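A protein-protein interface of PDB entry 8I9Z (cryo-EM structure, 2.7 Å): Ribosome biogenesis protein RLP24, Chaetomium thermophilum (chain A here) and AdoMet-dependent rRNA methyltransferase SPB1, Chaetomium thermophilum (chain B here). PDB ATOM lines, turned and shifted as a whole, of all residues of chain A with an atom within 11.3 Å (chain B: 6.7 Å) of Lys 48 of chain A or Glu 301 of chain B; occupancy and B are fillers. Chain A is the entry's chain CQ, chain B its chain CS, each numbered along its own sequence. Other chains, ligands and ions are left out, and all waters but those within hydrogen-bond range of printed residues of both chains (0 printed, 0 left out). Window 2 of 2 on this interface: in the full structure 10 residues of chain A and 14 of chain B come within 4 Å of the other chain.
ND2 of Asn 45 of chain A sits at hydrogen-bond distance from OD1 of Asp 316 of chain B (3.0 Å).
OE1 of Glu 301 of chain B is in salt-bridge range of NH1 of Arg 47 of chain A (3.6 Å).
The side-chain amino group (NZ) of Lys 48 of chain A is in salt-bridge range of the side-chain carboxylate (OE2) of Glu 301 of chain B (3.4 Å).
The side-chain amino group of Lys 300 of chain B lies within hydrogen-bond range of the side-chain amide oxygen of Asn 58 of chain A, 3.3 Å away.
The side-chain amide oxygen (OD1) of Asn 45 of chain A lies within hydrogen-bond range of the guanidinium group (NH2) of Arg 47 of chain A (2.9 Å).
The backbone carbonyl oxygen (O) of Glu 301 of chain B is in hydrogen-bond range of the side-chain sulfur (SG) of Cys 305 of chain B, 3.2 Å away.
SG of Cys 305 of chain B sits at hydrogen-bond distance from OD1 of Asp 316 of chain B (3.6 Å).
Among the printed residues, pairs that only touch across the chains: Asn 45 of chain A with Glu 301 of chain B and Arg 47 of chain A with Ala 304 of chain B.
Of the printed residues of chain B, Asn 45 of chain A touches Glu 301 (3.6 Å) and Asp 316 (3.0 Å).
Of the printed residues of chain B, Arg 47 of chain A touches Glu 301 (3.6 Å) and Ala 304 (3.4 Å).
Lys 48 of chain A touches one residue of chain B.
Trp 51 of chain A touches none of the printed residues of chain B.
Of the printed residues of chain B, Asn 58 of chain A touches Lys 300 (3.3 Å).
Thr 298 of chain B touches none of the printed residues of chain A.
Printed residues of chain A within 4 Å of Lys 300 of chain B: Asn 58 (3.3 Å).
Of the printed residues of chain A, Asp 316 of chain B touches Asn 45.
The nearest residue of chain A that does not touch Glu 301 of chain B is Asn 58 of chain A (5.0 Å).
Printed residues of chain A that touch a printed residue of chain B: Asn 45, Arg 47, Lys 48 and Asn 58.
Of the 13 printed residues of chain B, 4 touch a printed residue of chain A.
Hydrophobic or aromatic side chains of chain B within 4 Å of the printed part of chain A: Ala 304.
Along chain B the printed residues that touch a printed residue of chain A span positions 300 to 316.
Among the printed residues, Asp or Glu carboxylates within 4 Å of a Lys or Arg side-chain nitrogen of the other chain: Arg 47 of chain A with Glu 301 of chain B and Lys 48 of chain A with Glu 301 of chain B.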
ATOM      1  N   PHE A   7     -22.147 -22.005  -6.123  1.00  0.00           N
ATOM      2  CA  PHE A   7     -21.634 -20.704  -5.710  1.00  0.00           C
ATOM      3  C   PHE A   7     -20.403 -20.848  -4.827  1.00  0.00           C
ATOM      4  O   PHE A   7     -19.463 -20.052  -4.926  1.00  0.00           O
ATOM      5  CB  PHE A   7     -22.723 -19.917  -4.984  1.00  0.00           C
ATOM      6  CG  PHE A   7     -22.278 -18.570  -4.497  1.00  0.00           C
ATOM      7  CD1 PHE A   7     -22.144 -17.516  -5.376  1.00  0.00           C
ATOM      8  CD2 PHE A   7     -21.998 -18.359  -3.160  1.00  0.00           C
ATOM      9  CE1 PHE A   7     -21.735 -16.278  -4.935  1.00  0.00           C
ATOM     10  CE2 PHE A   7     -21.589 -17.123  -2.713  1.00  0.00           C
ATOM     11  CZ  PHE A   7     -21.458 -16.082  -3.601  1.00  0.00           C
ATOM     12  N   PHE A   8     -20.389 -21.853  -3.957  1.00  0.00           N
ATOM     13  CA  PHE A   8     -19.317 -22.011  -2.987  1.00  0.00           C
ATOM     14  C   PHE A   8     -18.064 -22.636  -3.588  1.00  0.00           C
ATOM     15  O   PHE A   8     -16.962 -22.112  -3.407  1.00  0.00           O
ATOM     16  CB  PHE A   8     -19.800 -22.853  -1.805  1.00  0.00           C
ATOM     17  CG  PHE A   8     -19.062 -22.585  -0.533  1.00  0.00           C
ATOM     18  CD1 PHE A   8     -17.905 -23.278  -0.231  1.00  0.00           C
ATOM     19  CD2 PHE A   8     -19.526 -21.645   0.366  1.00  0.00           C
ATOM     20  CE1 PHE A   8     -17.222 -23.035   0.937  1.00  0.00           C
ATOM     21  CE2 PHE A   8     -18.845 -21.400   1.538  1.00  0.00           C
ATOM     22  CZ  PHE A   8     -17.691 -22.096   1.822  1.00  0.00           C
ATOM     23  N   CYS A   9     -18.211 -23.751  -4.299  1.00  0.00           N
ATOM     24  CA  CYS A   9     -17.067 -24.554  -4.695  1.00  0.00           C
ATOM     25  C   CYS A   9     -16.945 -24.794  -6.193  1.00  0.00           C
ATOM     26  O   CYS A   9     -15.872 -25.206  -6.645  1.00  0.00           O
ATOM     27  CB  CYS A   9     -17.112 -25.897  -3.965  1.00  0.00           C
ATOM     28  SG  CYS A   9     -18.389 -26.950  -4.587  1.00  0.00           S
ATOM     29  N   ASN A  39     -21.587 -24.611   5.120  1.00  0.00           N
ATOM     30  CA  ASN A  39     -20.432 -23.731   5.240  1.00  0.00           C
ATOM     31  C   ASN A  39     -20.758 -22.296   4.851  1.00  0.00           C
ATOM     32  O   ASN A  39     -20.119 -21.368   5.355  1.00  0.00           O
ATOM     33  CB  ASN A  39     -19.290 -24.254   4.374  1.00  0.00           C
ATOM     34  CG  ASN A  39     -18.554 -25.400   5.016  1.00  0.00           C
ATOM     35  OD1 ASN A  39     -18.283 -25.386   6.215  1.00  0.00           O
ATOM     36  ND2 ASN A  39     -18.223 -26.405   4.224  1.00  0.00           N
ATOM     37  N   LYS A  43     -20.947 -18.693   7.307  1.00  0.00           N
ATOM     38  CA  LYS A  43     -20.240 -17.524   6.782  1.00  0.00           C
ATOM     39  C   LYS A  43     -18.732 -17.733   6.772  1.00  0.00           C
ATOM     40  O   LYS A  43     -17.961 -16.929   7.297  1.00  0.00           O
ATOM     41  CB  LYS A  43     -20.622 -16.261   7.551  1.00  0.00           C
ATOM     42  CG  LYS A  43     -22.108 -16.000   7.526  1.00  0.00           C
ATOM     43  CD  LYS A  43     -22.445 -14.627   8.040  1.00  0.00           C
ATOM     44  CE  LYS A  43     -23.487 -13.964   7.160  1.00  0.00           C
ATOM     45  NZ  LYS A  43     -24.862 -14.207   7.666  1.00  0.00           N
ATOM     46  N   ARG A  44     -18.318 -18.837   6.176  1.00  0.00           N
ATOM     47  CA  ARG A  44     -16.904 -19.080   5.982  1.00  0.00           C
ATOM     48  C   ARG A  44     -16.527 -18.660   4.565  1.00  0.00           C
ATOM     49  O   ARG A  44     -17.359 -18.639   3.658  1.00  0.00           O
ATOM     50  CB  ARG A  44     -16.581 -20.547   6.241  1.00  0.00           C
ATOM     51  CG  ARG A  44     -15.105 -20.808   6.503  1.00  0.00           C
ATOM     52  CD  ARG A  44     -14.777 -22.153   7.210  1.00  0.00           C
ATOM     53  NE  ARG A  44     -15.759 -22.820   8.074  1.00  0.00           N
ATOM     54  CZ  ARG A  44     -16.459 -22.292   9.077  1.00  0.00           C
ATOM     55  NH1 ARG A  44     -16.301 -21.035   9.464  1.00  0.00           N
ATOM     56  NH2 ARG A  44     -17.316 -23.062   9.738  1.00  0.00           N
ATOM     57  N   ASN A  45     -15.257 -18.307   4.379  1.00  0.00           N
ATOM     58  CA  ASN A  45     -14.818 -17.714   3.126  1.00  0.00           C
ATOM     59  C   ASN A  45     -14.284 -18.786   2.192  1.00  0.00           C
ATOM     60  O   ASN A  45     -13.248 -19.391   2.495  1.00  0.00           O
ATOM     61  CB  ASN A  45     -13.749 -16.659   3.386  1.00  0.00           C
ATOM     62  CG  ASN A  45     -13.756 -15.569   2.348  1.00  0.00           C
ATOM     63  OD1 ASN A  45     -14.589 -15.568   1.446  1.00  0.00           O
ATOM     64  ND2 ASN A  45     -12.814 -14.644   2.454  1.00  0.00           N
ATOM     65  N   PRO A  46     -14.922 -19.030   1.044  1.00  0.00           N
ATOM     66  CA  PRO A  46     -14.472 -20.121   0.163  1.00  0.00           C
ATOM     67  C   PRO A  46     -13.112 -19.896  -0.477  1.00  0.00           C
ATOM     68  O   PRO A  46     -12.503 -20.859  -0.961  1.00  0.00           O
ATOM     69  CB  PRO A  46     -15.592 -20.198  -0.882  1.00  0.00           C
ATOM     70  CG  PRO A  46     -16.234 -18.876  -0.851  1.00  0.00           C
ATOM     71  CD  PRO A  46     -16.166 -18.415   0.560  1.00  0.00           C
ATOM     72  N   ARG A  47     -12.608 -18.662  -0.487  1.00  0.00           N
ATOM     73  CA  ARG A  47     -11.266 -18.418  -1.009  1.00  0.00           C
ATOM     74  C   ARG A  47     -10.188 -18.994  -0.100  1.00  0.00           C
ATOM     75  O   ARG A  47      -9.047 -19.181  -0.537  1.00  0.00           O
ATOM     76  CB  ARG A  47     -11.060 -16.920  -1.221  1.00  0.00           C
ATOM     77  CG  ARG A  47     -11.609 -16.421  -2.541  1.00  0.00           C
ATOM     78  CD  ARG A  47     -12.020 -14.975  -2.469  1.00  0.00           C
ATOM     79  NE  ARG A  47     -13.416 -14.832  -2.079  1.00  0.00           N
ATOM     80  CZ  ARG A  47     -13.854 -13.994  -1.153  1.00  0.00           C
ATOM     81  NH1 ARG A  47     -13.027 -13.215  -0.479  1.00  0.00           N
ATOM     82  NH2 ARG A  47     -15.156 -13.939  -0.894  1.00  0.00           N
ATOM     83  N   LYS A  48     -10.522 -19.283   1.156  1.00  0.00           N
ATOM     84  CA  LYS A  48      -9.578 -19.841   2.115  1.00  0.00           C
ATOM     85  C   LYS A  48      -9.668 -21.358   2.233  1.00  0.00           C
ATOM     86  O   LYS A  48      -8.666 -22.005   2.552  1.00  0.00           O
ATOM     87  CB  LYS A  48      -9.791 -19.197   3.486  1.00  0.00           C
ATOM     88  CG  LYS A  48     -10.142 -17.723   3.416  1.00  0.00           C
ATOM     89  CD  LYS A  48      -9.549 -16.956   4.589  1.00  0.00           C
ATOM     90  CE  LYS A  48      -8.094 -16.606   4.332  1.00  0.00           C
ATOM     91  NZ  LYS A  48      -7.881 -16.127   2.941  1.00  0.00           N
ATOM     92  N   LEU A  49     -10.840 -21.944   1.997  1.00  0.00           N
ATOM     93  CA  LEU A  49     -10.953 -23.397   2.040  1.00  0.00           C
ATOM     94  C   LEU A  49     -10.288 -23.998   0.813  1.00  0.00           C
ATOM     95  O   LEU A  49     -10.580 -23.609  -0.321  1.00  0.00           O
ATOM     96  CB  LEU A  49     -12.411 -23.849   2.107  1.00  0.00           C
ATOM     97  CG  LEU A  49     -13.206 -23.766   3.410  1.00  0.00           C
ATOM     98  CD1 LEU A  49     -12.360 -24.178   4.614  1.00  0.00           C
ATOM     99  CD2 LEU A  49     -13.823 -22.421   3.580  1.00  0.00           C
ATOM    100  N   LYS A  50      -9.410 -24.966   1.040  1.00  0.00           N
ATOM    101  CA  LYS A  50      -8.531 -25.456  -0.007  1.00  0.00           C
ATOM    102  C   LYS A  50      -9.209 -26.427  -0.962  1.00  0.00           C
ATOM    103  O   LYS A  50      -8.593 -26.822  -1.956  1.00  0.00           O
ATOM    104  CB  LYS A  50      -7.299 -26.094   0.636  1.00  0.00           C
ATOM    105  CG  LYS A  50      -6.628 -25.173   1.645  1.00  0.00           C
ATOM    106  CD  LYS A  50      -5.296 -25.708   2.140  1.00  0.00           C
ATOM    107  CE  LYS A  50      -4.976 -25.147   3.521  1.00  0.00           C
ATOM    108  NZ  LYS A  50      -4.438 -26.162   4.473  1.00  0.00           N
ATOM    109  N   TRP A  51     -10.452 -26.819  -0.702  1.00  0.00           N
ATOM    110  CA  TRP A  51     -11.168 -27.715  -1.596  1.00  0.00           C
ATOM    111  C   TRP A  51     -12.049 -26.970  -2.590  1.00  0.00           C
ATOM    112  O   TRP A  51     -12.528 -27.577  -3.550  1.00  0.00           O
ATOM    113  CB  TRP A  51     -12.002 -28.717  -0.790  1.00  0.00           C
ATOM    114  CG  TRP A  51     -12.836 -28.117   0.304  1.00  0.00           C
ATOM    115  CD1 TRP A  51     -12.431 -27.806   1.561  1.00  0.00           C
ATOM    116  CD2 TRP A  51     -14.227 -27.796   0.243  1.00  0.00           C
ATOM    117  NE1 TRP A  51     -13.472 -27.291   2.284  1.00  0.00           N
ATOM    118  CE2 TRP A  51     -14.589 -27.278   1.497  1.00  0.00           C
ATOM    119  CE3 TRP A  51     -15.200 -27.892  -0.753  1.00  0.00           C
ATOM    120  CZ2 TRP A  51     -15.876 -26.855   1.781  1.00  0.00           C
ATOM    121  CZ3 TRP A  51     -16.475 -27.472  -0.469  1.00  0.00           C
ATOM    122  CH2 TRP A  51     -16.804 -26.958   0.788  1.00  0.00           C
ATOM    123  N   THR A  52     -12.247 -25.670  -2.401  1.00  0.00           N
ATOM    124  CA  THR A  52     -13.084 -24.867  -3.278  1.00  0.00           C
ATOM    125  C   THR A  52     -12.274 -24.408  -4.481  1.00  0.00           C
ATOM    126  O   THR A  52     -11.048 -24.303  -4.410  1.00  0.00           O
ATOM    127  CB  THR A  52     -13.650 -23.654  -2.539  1.00  0.00           C
ATOM    128  OG1 THR A  52     -12.594 -22.724  -2.279  1.00  0.00           O
ATOM    129  CG2 THR A  52     -14.275 -24.075  -1.229  1.00  0.00           C
ATOM    130  N   LYS A  53     -12.965 -24.147  -5.592  1.00  0.00           N
ATOM    131  CA  LYS A  53     -12.271 -23.713  -6.796  1.00  0.00           C
ATOM    132  C   LYS A  53     -11.903 -22.240  -6.753  1.00  0.00           C
ATOM    133  O   LYS A  53     -11.068 -21.800  -7.550  1.00  0.00           O
ATOM    134  CB  LYS A  53     -13.109 -24.005  -8.038  1.00  0.00           C
ATOM    135  CG  LYS A  53     -13.051 -25.445  -8.486  1.00  0.00           C
ATOM    136  CD  LYS A  53     -11.904 -25.635  -9.457  1.00  0.00           C
ATOM    137  CE  LYS A  53     -12.163 -26.763 -10.428  1.00  0.00           C
ATOM    138  NZ  LYS A  53     -11.174 -27.862 -10.282  1.00  0.00           N
ATOM    139  N   ALA A  54     -12.511 -21.470  -5.854  1.00  0.00           N
ATOM    140  CA  ALA A  54     -12.116 -20.077  -5.685  1.00  0.00           C
ATOM    141  C   ALA A  54     -10.700 -19.979  -5.134  1.00  0.00           C
ATOM    142  O   ALA A  54      -9.938 -19.079  -5.502  1.00  0.00           O
ATOM    143  CB  ALA A  54     -13.107 -19.359  -4.771  1.00  0.00           C
ATOM    144  N   TYR A  55     -10.338 -20.900  -4.237  1.00  0.00           N
ATOM    145  CA  TYR A  55      -8.982 -20.938  -3.703  1.00  0.00           C
ATOM    146  C   TYR A  55      -7.980 -21.349  -4.770  1.00  0.00           C
ATOM    147  O   TYR A  55      -6.879 -20.793  -4.842  1.00  0.00           O
ATOM    148  CB  TYR A  55      -8.926 -21.896  -2.513  1.00  0.00           C
ATOM    149  CG  TYR A  55      -7.541 -22.302  -2.056  1.00  0.00           C
ATOM    150  CD1 TYR A  55      -6.821 -21.505  -1.183  1.00  0.00           C
ATOM    151  CD2 TYR A  55      -6.963 -23.493  -2.484  1.00  0.00           C
ATOM    152  CE1 TYR A  55      -5.566 -21.873  -0.757  1.00  0.00           C
ATOM    153  CE2 TYR A  55      -5.712 -23.866  -2.064  1.00  0.00           C
ATOM    154  CZ  TYR A  55      -5.016 -23.053  -1.202  1.00  0.00           C
ATOM    155  OH  TYR A  55      -3.762 -23.423  -0.780  1.00  0.00           O
ATOM    156  N   ARG A  56      -8.338 -22.336  -5.591  1.00  0.00           N
ATOM    157  CA  ARG A  56      -7.412 -22.864  -6.588  1.00  0.00           C
ATOM    158  C   ARG A  56      -7.101 -21.825  -7.658  1.00  0.00           C
ATOM    159  O   ARG A  56      -5.966 -21.731  -8.139  1.00  0.00           O
ATOM    160  CB  ARG A  56      -7.996 -24.122  -7.215  1.00  0.00           C
ATOM    161  CG  ARG A  56      -8.416 -25.183  -6.225  1.00  0.00           C
ATOM    162  CD  ARG A  56      -8.355 -26.548  -6.859  1.00  0.00           C
ATOM    163  NE  ARG A  56      -7.024 -27.129  -6.771  1.00  0.00           N
ATOM    164  CZ  ARG A  56      -6.451 -27.826  -7.740  1.00  0.00           C
ATOM    165  NH1 ARG A  56      -7.048 -28.008  -8.903  1.00  0.00           N
ATOM    166  NH2 ARG A  56      -5.246 -28.349  -7.537  1.00  0.00           N
ATOM    167  N   LYS A  57      -8.107 -21.045  -8.053  1.00  0.00           N
ATOM    168  CA  LYS A  57      -7.870 -19.935  -8.967  1.00  0.00           C
ATOM    169  C   LYS A  57      -7.054 -18.836  -8.298  1.00  0.00           C
ATOM    170  O   LYS A  57      -6.199 -18.211  -8.934  1.00  0.00           O
ATOM    171  CB  LYS A  57      -9.202 -19.380  -9.468  1.00  0.00           C
ATOM    172  CG  LYS A  57      -9.953 -20.313 -10.391  1.00  0.00           C
ATOM    173  CD  LYS A  57     -11.021 -19.572 -11.171  1.00  0.00           C
ATOM    174  CE  LYS A  57     -12.415 -20.015 -10.759  1.00  0.00           C
ATOM    175  NZ  LYS A  57     -12.550 -20.127  -9.281  1.00  0.00           N
ATOM    176  N   ASN A  58      -7.313 -18.582  -7.015  1.00  0.00           N
ATOM    177  CA  ASN A  58      -6.577 -17.551  -6.296  1.00  0.00           C
ATOM    178  C   ASN A  58      -5.135 -17.972  -6.043  1.00  0.00           C
ATOM    179  O   ASN A  58      -4.227 -17.133  -6.050  1.00  0.00           O
ATOM    180  CB  ASN A  58      -7.281 -17.231  -4.978  1.00  0.00           C
ATOM    181  CG  ASN A  58      -7.371 -15.745  -4.711  1.00  0.00           C
ATOM    182  OD1 ASN A  58      -7.597 -14.951  -5.623  1.00  0.00           O
ATOM    183  ND2 ASN A  58      -7.202 -15.361  -3.451  1.00  0.00           N
ATOM    184  N   ALA A  59      -4.903 -19.261  -5.812  1.00  0.00           N
ATOM    185  CA  ALA A  59      -3.564 -19.756  -5.530  1.00  0.00           C
ATOM    186  C   ALA A  59      -2.800 -20.176  -6.777  1.00  0.00           C
ATOM    187  O   ALA A  59      -1.630 -20.554  -6.666  1.00  0.00           O
ATOM    188  CB  ALA A  59      -3.625 -20.935  -4.555  1.00  0.00           C
ATOM    189  N   LYS A  61      -3.468 -22.765  -8.911  1.00  0.00           N
ATOM    190  CA  LYS A  61      -3.381 -24.203  -9.117  1.00  0.00           C
ATOM    191  C   LYS A  61      -4.058 -24.668 -10.399  1.00  0.00           C
ATOM    192  O   LYS A  61      -3.838 -25.810 -10.812  1.00  0.00           O
ATOM    193  CB  LYS A  61      -3.962 -24.923  -7.905  1.00  0.00           C
ATOM    194  CG  LYS A  61      -3.177 -24.614  -6.644  1.00  0.00           C
ATOM    195  CD  LYS A  61      -3.804 -25.206  -5.409  1.00  0.00           C
ATOM    196  CE  LYS A  61      -3.009 -24.804  -4.181  1.00  0.00           C
ATOM    197  NZ  LYS A  61      -1.650 -25.402  -4.192  1.00  0.00           N
ATOM    198  N   THR B 298      -5.269  -3.147  -0.249  1.00  0.00           N
ATOM    199  CA  THR B 298      -6.549  -3.534  -0.858  1.00  0.00           C
ATOM    200  C   THR B 298      -6.390  -4.336  -2.147  1.00  0.00           C
ATOM    201  O   THR B 298      -6.881  -3.941  -3.209  1.00  0.00           O
ATOM    202  CB  THR B 298      -7.503  -2.331  -1.079  1.00  0.00           C
ATOM    203  OG1 THR B 298      -8.638  -2.756  -1.845  1.00  0.00           O
ATOM    204  CG2 THR B 298      -6.875  -1.101  -1.754  1.00  0.00           C
ATOM    205  N   THR B 299      -5.710  -5.474  -2.053  1.00  0.00           N
ATOM    206  CA  THR B 299      -5.478  -6.350  -3.191  1.00  0.00           C
ATOM    207  C   THR B 299      -6.309  -7.610  -3.021  1.00  0.00           C
ATOM    208  O   THR B 299      -6.210  -8.282  -1.988  1.00  0.00           O
ATOM    209  CB  THR B 299      -3.996  -6.705  -3.320  1.00  0.00           C
ATOM    210  OG1 THR B 299      -3.543  -7.312  -2.103  1.00  0.00           O
ATOM    211  CG2 THR B 299      -3.170  -5.456  -3.598  1.00  0.00           C
ATOM    212  N   LYS B 300      -7.148  -7.901  -4.019  1.00  0.00           N
ATOM    213  CA  LYS B 300      -7.874  -9.162  -4.162  1.00  0.00           C
ATOM    214  C   LYS B 300      -8.846  -9.436  -3.020  1.00  0.00           C
ATOM    215  O   LYS B 300     -10.062  -9.421  -3.228  1.00  0.00           O
ATOM    216  CB  LYS B 300      -6.899 -10.333  -4.313  1.00  0.00           C
ATOM    217  CG  LYS B 300      -5.942 -10.187  -5.479  1.00  0.00           C
ATOM    218  CD  LYS B 300      -6.701 -10.084  -6.792  1.00  0.00           C
ATOM    219  CE  LYS B 300      -7.359 -11.405  -7.151  1.00  0.00           C
ATOM    220  NZ  LYS B 300      -6.354 -12.469  -7.419  1.00  0.00           N
ATOM    221  N   GLU B 301      -8.319  -9.705  -1.823  1.00  0.00           N
ATOM    222  CA  GLU B 301      -9.169 -10.102  -0.704  1.00  0.00           C
ATOM    223  C   GLU B 301     -10.074  -8.962  -0.251  1.00  0.00           C
ATOM    224  O   GLU B 301     -11.244  -9.182   0.080  1.00  0.00           O
ATOM    225  CB  GLU B 301      -8.313 -10.606   0.457  1.00  0.00           C
ATOM    226  CG  GLU B 301      -8.144 -12.118   0.482  1.00  0.00           C
ATOM    227  CD  GLU B 301      -9.383 -12.843   0.979  1.00  0.00           C
ATOM    228  OE1 GLU B 301     -10.260 -12.190   1.587  1.00  0.00           O
ATOM    229  OE2 GLU B 301      -9.484 -14.068   0.759  1.00  0.00           O
ATOM    230  N   ILE B 302      -9.548  -7.736  -0.222  1.00  0.00           N
ATOM    231  CA  ILE B 302     -10.381  -6.590   0.133  1.00  0.00           C
ATOM    232  C   ILE B 302     -11.411  -6.330  -0.956  1.00  0.00           C
ATOM    233  O   ILE B 302     -12.582  -6.047  -0.672  1.00  0.00           O
ATOM    234  CB  ILE B 302      -9.506  -5.353   0.402  1.00  0.00           C
ATOM    235  CG1 ILE B 302      -8.587  -5.602   1.593  1.00  0.00           C
ATOM    236  CG2 ILE B 302     -10.363  -4.126   0.668  1.00  0.00           C
ATOM    237  CD1 ILE B 302      -9.331  -5.830   2.875  1.00  0.00           C
ATOM    238  N   ARG B 303     -10.996  -6.442  -2.217  1.00  0.00           N
ATOM    239  CA  ARG B 303     -11.902  -6.189  -3.330  1.00  0.00           C
ATOM    240  C   ARG B 303     -13.002  -7.241  -3.402  1.00  0.00           C
ATOM    241  O   ARG B 303     -14.138  -6.937  -3.785  1.00  0.00           O
ATOM    242  CB  ARG B 303     -11.111  -6.144  -4.635  1.00  0.00           C
ATOM    243  CG  ARG B 303     -11.791  -5.379  -5.747  1.00  0.00           C
ATOM    244  CD  ARG B 303     -11.597  -3.885  -5.564  1.00  0.00           C
ATOM    245  NE  ARG B 303     -12.171  -3.127  -6.667  1.00  0.00           N
ATOM    246  CZ  ARG B 303     -11.524  -2.829  -7.785  1.00  0.00           C
ATOM    247  NH1 ARG B 303     -10.275  -3.215  -7.983  1.00  0.00           N
ATOM    248  NH2 ARG B 303     -12.147  -2.129  -8.729  1.00  0.00           N
ATOM    249  N   ALA B 304     -12.684  -8.485  -3.043  1.00  0.00           N
ATOM    250  CA  ALA B 304     -13.698  -9.534  -3.035  1.00  0.00           C
ATOM    251  C   ALA B 304     -14.666  -9.368  -1.870  1.00  0.00           C
ATOM    252  O   ALA B 304     -15.864  -9.634  -2.011  1.00  0.00           O
ATOM    253  CB  ALA B 304     -13.033 -10.908  -2.989  1.00  0.00           C
ATOM    254  N   CYS B 305     -14.167  -8.939  -0.709  1.00  0.00           N
ATOM    255  CA  CYS B 305     -15.045  -8.725   0.438  1.00  0.00           C
ATOM    256  C   CYS B 305     -15.923  -7.497   0.245  1.00  0.00           C
ATOM    257  O   CYS B 305     -17.043  -7.440   0.766  1.00  0.00           O
ATOM    258  CB  CYS B 305     -14.222  -8.593   1.719  1.00  0.00           C
ATOM    259  SG  CYS B 305     -13.418 -10.111   2.267  1.00  0.00           S
ATOM    260  N   CYS B 306     -15.433  -6.499  -0.495  1.00  0.00           N
ATOM    261  CA  CYS B 306     -16.206  -5.276  -0.691  1.00  0.00           C
ATOM    262  C   CYS B 306     -17.352  -5.475  -1.673  1.00  0.00           C
ATOM    263  O   CYS B 306     -18.294  -4.676  -1.692  1.00  0.00           O
ATOM    264  CB  CYS B 306     -15.296  -4.144  -1.164  1.00  0.00           C
ATOM    265  SG  CYS B 306     -14.296  -3.402   0.139  1.00  0.00           S
ATOM    266  N   LYS B 315     -13.515 -12.748  10.429  1.00  0.00           N
ATOM    267  CA  LYS B 315     -12.176 -12.395   9.971  1.00  0.00           C
ATOM    268  C   LYS B 315     -12.232 -11.456   8.776  1.00  0.00           C
ATOM    269  O   LYS B 315     -11.312 -10.659   8.564  1.00  0.00           O
ATOM    270  CB  LYS B 315     -11.380 -13.654   9.624  1.00  0.00           C
ATOM    271  CG  LYS B 315     -10.686 -14.354  10.798  1.00  0.00           C
ATOM    272  CD  LYS B 315     -11.643 -15.036  11.754  1.00  0.00           C
ATOM    273  CE  LYS B 315     -10.896 -15.679  12.907  1.00  0.00           C
ATOM    274  NZ  LYS B 315      -9.607 -16.274  12.461  1.00  0.00           N
ATOM    275  N   ASP B 316     -13.297 -11.538   7.982  1.00  0.00           N
ATOM    276  CA  ASP B 316     -13.421 -10.654   6.831  1.00  0.00           C
ATOM    277  C   ASP B 316     -13.811  -9.246   7.256  1.00  0.00           C
ATOM    278  O   ASP B 316     -13.328  -8.264   6.681  1.00  0.00           O
ATOM    279  CB  ASP B 316     -14.431 -11.227   5.844  1.00  0.00           C
ATOM    280  CG  ASP B 316     -13.983 -12.549   5.263  1.00  0.00           C
ATOM    281  OD1 ASP B 316     -14.498 -12.940   4.194  1.00  0.00           O
ATOM    282  OD2 ASP B 316     -13.115 -13.201   5.877  1.00  0.00           O
ATOM    283  N   LEU B 319     -10.695  -7.682   8.906  1.00  0.00           N
ATOM    284  CA  LEU B 319      -9.661  -7.305   7.949  1.00  0.00           C
ATOM    285  C   LEU B 319     -10.035  -6.011   7.233  1.00  0.00           C
ATOM    286  O   LEU B 319      -9.160  -5.208   6.891  1.00  0.00           O
ATOM    287  CB  LEU B 319      -9.446  -8.457   6.964  1.00  0.00           C
ATOM    288  CG  LEU B 319      -8.804  -8.413   5.573  1.00  0.00           C
ATOM    289  CD1 LEU B 319      -7.503  -7.613   5.530  1.00  0.00           C
ATOM    290  CD2 LEU B 319      -8.568  -9.827   5.079  1.00  0.00           C
ATOM    291  N   LEU B 320     -11.333  -5.784   7.016  1.00  0.00           N
ATOM    292  CA  LEU B 320     -11.779  -4.511   6.458  1.00  0.00           C
ATOM    293  C   LEU B 320     -11.528  -3.362   7.427  1.00  0.00           C
ATOM    294  O   LEU B 320     -11.180  -2.252   7.007  1.00  0.00           O
ATOM    295  CB  LEU B 320     -13.262  -4.579   6.094  1.00  0.00           C
ATOM    296  CG  LEU B 320     -13.641  -5.278   4.790  1.00  0.00           C
ATOM    297  CD1 LEU B 320     -15.122  -5.128   4.520  1.00  0.00           C
ATOM    298  CD2 LEU B 320     -12.838  -4.725   3.634  1.00  0.00           C
